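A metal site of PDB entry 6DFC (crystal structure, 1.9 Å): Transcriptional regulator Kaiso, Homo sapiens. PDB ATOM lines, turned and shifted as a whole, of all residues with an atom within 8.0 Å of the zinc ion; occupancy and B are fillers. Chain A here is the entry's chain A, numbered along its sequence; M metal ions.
O of Lys 59 is in hydrogen-bond range of N of Cys 54 (2.8 Å). The side-chain sulfur of Cys 54 lies close to the backbone NH of Tyr 56 (3.3 Å). The side-chain sulfur of Cys 57 sits close to the backbone NH of Lys 59 (3.4 Å).
Within 4 Å of the zinc ion: Cys 54, Cys 57, His 70 and His 74. The nearest printed residue that does not touch the zinc ion is Tyr 56 (4.4 Å).
The zinc ion is bound by a ring nitrogen (NE2) of His 70 (2.1 Å), a ring nitrogen (NE2) of His 74 (2.1 Å), the side-chain sulfur (SG) of Cys 54 (2.2 Å) and the side-chain sulfur (SG) of Cys 57 (2.2 Å). The zinc ion has four donor atoms within binding distance.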
ATOM      1  N   PRO A  53     -26.188  -0.876 -20.668  1.00  0.00           N
ATOM      2  CA  PRO A  53     -25.486  -0.556 -19.426  1.00  0.00           C
ATOM      3  C   PRO A  53     -25.436  -1.731 -18.476  1.00  0.00           C
ATOM      4  O   PRO A  53     -26.434  -2.433 -18.341  1.00  0.00           O
ATOM      5  CB  PRO A  53     -26.327   0.574 -18.839  1.00  0.00           C
ATOM      6  CG  PRO A  53     -27.700   0.313 -19.360  1.00  0.00           C
ATOM      7  CD  PRO A  53     -27.500  -0.214 -20.749  1.00  0.00           C
ATOM      8  N   CYS A  54     -24.293  -1.955 -17.843  1.00  0.00           N
ATOM      9  CA  CYS A  54     -24.199  -2.967 -16.785  1.00  0.00           C
ATOM     10  C   CYS A  54     -25.130  -2.588 -15.627  1.00  0.00           C
ATOM     11  O   CYS A  54     -25.282  -1.415 -15.322  1.00  0.00           O
ATOM     12  CB  CYS A  54     -22.752  -3.112 -16.303  1.00  0.00           C
ATOM     13  SG  CYS A  54     -22.512  -4.201 -14.830  1.00  0.00           S
ATOM     14  N   ARG A  55     -25.787  -3.556 -15.009  1.00  0.00           N
ATOM     15  CA  ARG A  55     -26.736  -3.210 -13.956  1.00  0.00           C
ATOM     16  C   ARG A  55     -26.066  -3.125 -12.582  1.00  0.00           C
ATOM     17  O   ARG A  55     -26.698  -2.748 -11.616  1.00  0.00           O
ATOM     18  CB  ARG A  55     -27.895  -4.208 -13.920  1.00  0.00           C
ATOM     19  CG  ARG A  55     -27.578  -5.474 -13.113  1.00  0.00           C
ATOM     20  CD  ARG A  55     -28.704  -6.492 -13.139  1.00  0.00           C
ATOM     21  NE  ARG A  55     -28.781  -7.200 -14.419  1.00  0.00           N
ATOM     22  CZ  ARG A  55     -29.545  -8.269 -14.633  1.00  0.00           C
ATOM     23  NH1 ARG A  55     -30.284  -8.759 -13.652  1.00  0.00           N
ATOM     24  NH2 ARG A  55     -29.548  -8.848 -15.828  1.00  0.00           N
ATOM     25  N   TYR A  56     -24.783  -3.470 -12.508  1.00  0.00           N
ATOM     26  CA  TYR A  56     -24.069  -3.562 -11.227  1.00  0.00           C
ATOM     27  C   TYR A  56     -22.945  -2.537 -11.113  1.00  0.00           C
ATOM     28  O   TYR A  56     -22.519  -2.197 -10.026  1.00  0.00           O
ATOM     29  CB  TYR A  56     -23.466  -4.956 -11.030  1.00  0.00           C
ATOM     30  CG  TYR A  56     -24.468  -6.069 -11.010  1.00  0.00           C
ATOM     31  CD1 TYR A  56     -24.543  -6.968 -12.057  1.00  0.00           C
ATOM     32  CD2 TYR A  56     -25.332  -6.225  -9.941  1.00  0.00           C
ATOM     33  CE1 TYR A  56     -25.453  -8.002 -12.044  1.00  0.00           C
ATOM     34  CE2 TYR A  56     -26.246  -7.257  -9.915  1.00  0.00           C
ATOM     35  CZ  TYR A  56     -26.311  -8.141 -10.976  1.00  0.00           C
ATOM     36  OH  TYR A  56     -27.222  -9.169 -10.972  1.00  0.00           O
ATOM     37  N   CYS A  57     -22.441  -2.107 -12.253  1.00  0.00           N
ATOM     38  CA  CYS A  57     -21.523  -0.987 -12.293  1.00  0.00           C
ATOM     39  C   CYS A  57     -22.062  -0.184 -13.453  1.00  0.00           C
ATOM     40  O   CYS A  57     -23.098  -0.532 -14.007  1.00  0.00           O
ATOM     41  CB  CYS A  57     -20.075  -1.413 -12.499  1.00  0.00           C
ATOM     42  SG  CYS A  57     -19.662  -1.961 -14.140  1.00  0.00           S
ATOM     43  N   GLU A  58     -21.400   0.888 -13.848  1.00  0.00           N
ATOM     44  CA  GLU A  58     -21.991   1.582 -14.984  1.00  0.00           C
ATOM     45  C   GLU A  58     -21.069   1.584 -16.191  1.00  0.00           C
ATOM     46  O   GLU A  58     -20.928   2.578 -16.889  1.00  0.00           O
ATOM     47  CB  GLU A  58     -22.401   3.003 -14.588  1.00  0.00           C
ATOM     48  CG  GLU A  58     -23.679   3.097 -13.678  1.00  0.00           C
ATOM     49  CD  GLU A  58     -24.740   1.981 -13.863  1.00  0.00           C
ATOM     50  OE1 GLU A  58     -24.919   1.443 -14.985  1.00  0.00           O
ATOM     51  OE2 GLU A  58     -25.376   1.607 -12.854  1.00  0.00           O
ATOM     52  N   LYS A  59     -20.427   0.440 -16.440  1.00  0.00           N
ATOM     53  CA  LYS A  59     -19.848   0.200 -17.758  1.00  0.00           C
ATOM     54  C   LYS A  59     -21.003   0.077 -18.751  1.00  0.00           C
ATOM     55  O   LYS A  59     -22.099  -0.363 -18.396  1.00  0.00           O
ATOM     56  CB  LYS A  59     -18.972  -1.049 -17.777  1.00  0.00           C
ATOM     57  CG  LYS A  59     -17.691  -0.915 -16.957  1.00  0.00           C
ATOM     58  CD  LYS A  59     -16.990  -2.264 -16.826  1.00  0.00           C
ATOM     59  CE  LYS A  59     -16.049  -2.519 -17.986  1.00  0.00           C
ATOM     60  NZ  LYS A  59     -14.944  -1.522 -18.023  1.00  0.00           N
ATOM     61  N   VAL A  60     -20.766   0.474 -19.998  1.00  0.00           N
ATOM     62  CA  VAL A  60     -21.815   0.432 -21.009  1.00  0.00           C
ATOM     63  C   VAL A  60     -21.279  -0.314 -22.230  1.00  0.00           C
ATOM     64  O   VAL A  60     -20.139  -0.108 -22.631  1.00  0.00           O
ATOM     65  CB  VAL A  60     -22.296   1.849 -21.382  1.00  0.00           C
ATOM     66  CG1 VAL A  60     -23.378   1.789 -22.452  1.00  0.00           C
ATOM     67  CG2 VAL A  60     -22.792   2.571 -20.153  1.00  0.00           C
ATOM     68  N   PHE A  61     -22.090  -1.198 -22.801  1.00  0.00           N
ATOM     69  CA  PHE A  61     -21.640  -2.055 -23.903  1.00  0.00           C
ATOM     70  C   PHE A  61     -22.451  -1.805 -25.165  1.00  0.00           C
ATOM     71  O   PHE A  61     -23.622  -1.429 -25.075  1.00  0.00           O
ATOM     72  CB  PHE A  61     -21.738  -3.529 -23.497  1.00  0.00           C
ATOM     73  CG  PHE A  61     -20.896  -3.872 -22.309  1.00  0.00           C
ATOM     74  CD1 PHE A  61     -21.383  -3.652 -21.027  1.00  0.00           C
ATOM     75  CD2 PHE A  61     -19.630  -4.408 -22.456  1.00  0.00           C
ATOM     76  CE1 PHE A  61     -20.612  -3.959 -19.911  1.00  0.00           C
ATOM     77  CE2 PHE A  61     -18.855  -4.724 -21.346  1.00  0.00           C
ATOM     78  CZ  PHE A  61     -19.342  -4.492 -20.081  1.00  0.00           C
ATOM     79  N   ARG A  67     -22.649  -7.181 -22.634  1.00  0.00           N
ATOM     80  CA  ARG A  67     -23.147  -6.803 -21.321  1.00  0.00           C
ATOM     81  C   ARG A  67     -23.467  -8.027 -20.439  1.00  0.00           C
ATOM     82  O   ARG A  67     -23.059  -8.105 -19.268  1.00  0.00           O
ATOM     83  CB  ARG A  67     -24.394  -5.940 -21.436  1.00  0.00           C
ATOM     84  CG  ARG A  67     -24.988  -5.666 -20.024  1.00  0.00           C
ATOM     85  CD  ARG A  67     -26.192  -4.797 -20.052  1.00  0.00           C
ATOM     86  NE  ARG A  67     -27.304  -5.399 -20.761  1.00  0.00           N
ATOM     87  CZ  ARG A  67     -28.463  -4.779 -20.954  1.00  0.00           C
ATOM     88  NH1 ARG A  67     -28.632  -3.564 -20.465  1.00  0.00           N
ATOM     89  NH2 ARG A  67     -29.440  -5.370 -21.608  1.00  0.00           N
ATOM     90  N   HIS A  70     -20.450  -9.830 -19.107  1.00  0.00           N
ATOM     91  CA  HIS A  70     -19.904  -8.997 -18.055  1.00  0.00           C
ATOM     92  C   HIS A  70     -20.679  -9.085 -16.737  1.00  0.00           C
ATOM     93  O   HIS A  70     -20.074  -9.127 -15.662  1.00  0.00           O
ATOM     94  CB  HIS A  70     -19.879  -7.547 -18.525  1.00  0.00           C
ATOM     95  CG  HIS A  70     -19.498  -6.572 -17.463  1.00  0.00           C
ATOM     96  ND1 HIS A  70     -18.202  -6.420 -17.038  1.00  0.00           N
ATOM     97  CD2 HIS A  70     -20.247  -5.726 -16.728  1.00  0.00           C
ATOM     98  CE1 HIS A  70     -18.170  -5.491 -16.091  1.00  0.00           C
ATOM     99  NE2 HIS A  70     -19.389  -5.051 -15.899  1.00  0.00           N
ATOM    100  N   GLU A  71     -22.001  -9.097 -16.819  1.00  0.00           N
ATOM    101  CA  GLU A  71     -22.826  -9.123 -15.616  1.00  0.00           C
ATOM    102  C   GLU A  71     -22.642 -10.432 -14.873  1.00  0.00           C
ATOM    103  O   GLU A  71     -22.697 -10.474 -13.656  1.00  0.00           O
ATOM    104  CB  GLU A  71     -24.308  -8.917 -15.961  1.00  0.00           C
ATOM    105  CG  GLU A  71     -24.624  -7.438 -16.293  1.00  0.00           C
ATOM    106  CD  GLU A  71     -26.093  -7.175 -16.554  1.00  0.00           C
ATOM    107  OE1 GLU A  71     -26.807  -8.103 -16.962  1.00  0.00           O
ATOM    108  OE2 GLU A  71     -26.525  -6.026 -16.361  1.00  0.00           O
ATOM    109  N   ILE A  72     -22.403 -11.515 -15.622  1.00  0.00           N
ATOM    110  CA  ILE A  72     -22.166 -12.796 -14.956  1.00  0.00           C
ATOM    111  C   ILE A  72     -20.879 -12.743 -14.129  1.00  0.00           C
ATOM    112  O   ILE A  72     -20.793 -13.377 -13.074  1.00  0.00           O
ATOM    113  CB  ILE A  72     -22.133 -13.968 -15.979  1.00  0.00           C
ATOM    114  CG1 ILE A  72     -23.574 -14.321 -16.357  1.00  0.00           C
ATOM    115  CG2 ILE A  72     -21.493 -15.201 -15.377  1.00  0.00           C
ATOM    116  CD1 ILE A  72     -23.727 -14.991 -17.697  1.00  0.00           C
ATOM    117  N   HIS A  73     -19.890 -11.980 -14.583  1.00  0.00           N
ATOM    118  CA  HIS A  73     -18.674 -11.774 -13.787  1.00  0.00           C
ATOM    119  C   HIS A  73     -18.991 -11.116 -12.433  1.00  0.00           C
ATOM    120  O   HIS A  73     -18.348 -11.422 -11.424  1.00  0.00           O
ATOM    121  CB  HIS A  73     -17.662 -10.923 -14.554  1.00  0.00           C
ATOM    122  CG  HIS A  73     -16.624 -11.729 -15.275  1.00  0.00           C
ATOM    123  ND1 HIS A  73     -16.818 -12.213 -16.552  1.00  0.00           N
ATOM    124  CD2 HIS A  73     -15.395 -12.129 -14.902  1.00  0.00           C
ATOM    125  CE1 HIS A  73     -15.741 -12.882 -16.931  1.00  0.00           C
ATOM    126  NE2 HIS A  73     -14.858 -12.846 -15.947  1.00  0.00           N
ATOM    127  N   HIS A  74     -19.951 -10.198 -12.417  1.00  0.00           N
ATOM    128  CA  HIS A  74     -20.370  -9.599 -11.137  1.00  0.00           C
ATOM    129  C   HIS A  74     -20.963 -10.625 -10.160  1.00  0.00           C
ATOM    130  O   HIS A  74     -20.692 -10.568  -8.949  1.00  0.00           O
ATOM    131  CB  HIS A  74     -21.401  -8.496 -11.382  1.00  0.00           C
ATOM    132  CG  HIS A  74     -20.797  -7.181 -11.772  1.00  0.00           C
ATOM    133  ND1 HIS A  74     -20.122  -6.380 -10.885  1.00  0.00           N
ATOM    134  CD2 HIS A  74     -20.786  -6.512 -12.960  1.00  0.00           C
ATOM    135  CE1 HIS A  74     -19.728  -5.270 -11.494  1.00  0.00           C
ATOM    136  NE2 HIS A  74     -20.112  -5.338 -12.761  1.00  0.00           N
HETATM  137 ZN    ZN M   1     -20.380  -4.063 -14.400  1.00  0.00          ZN
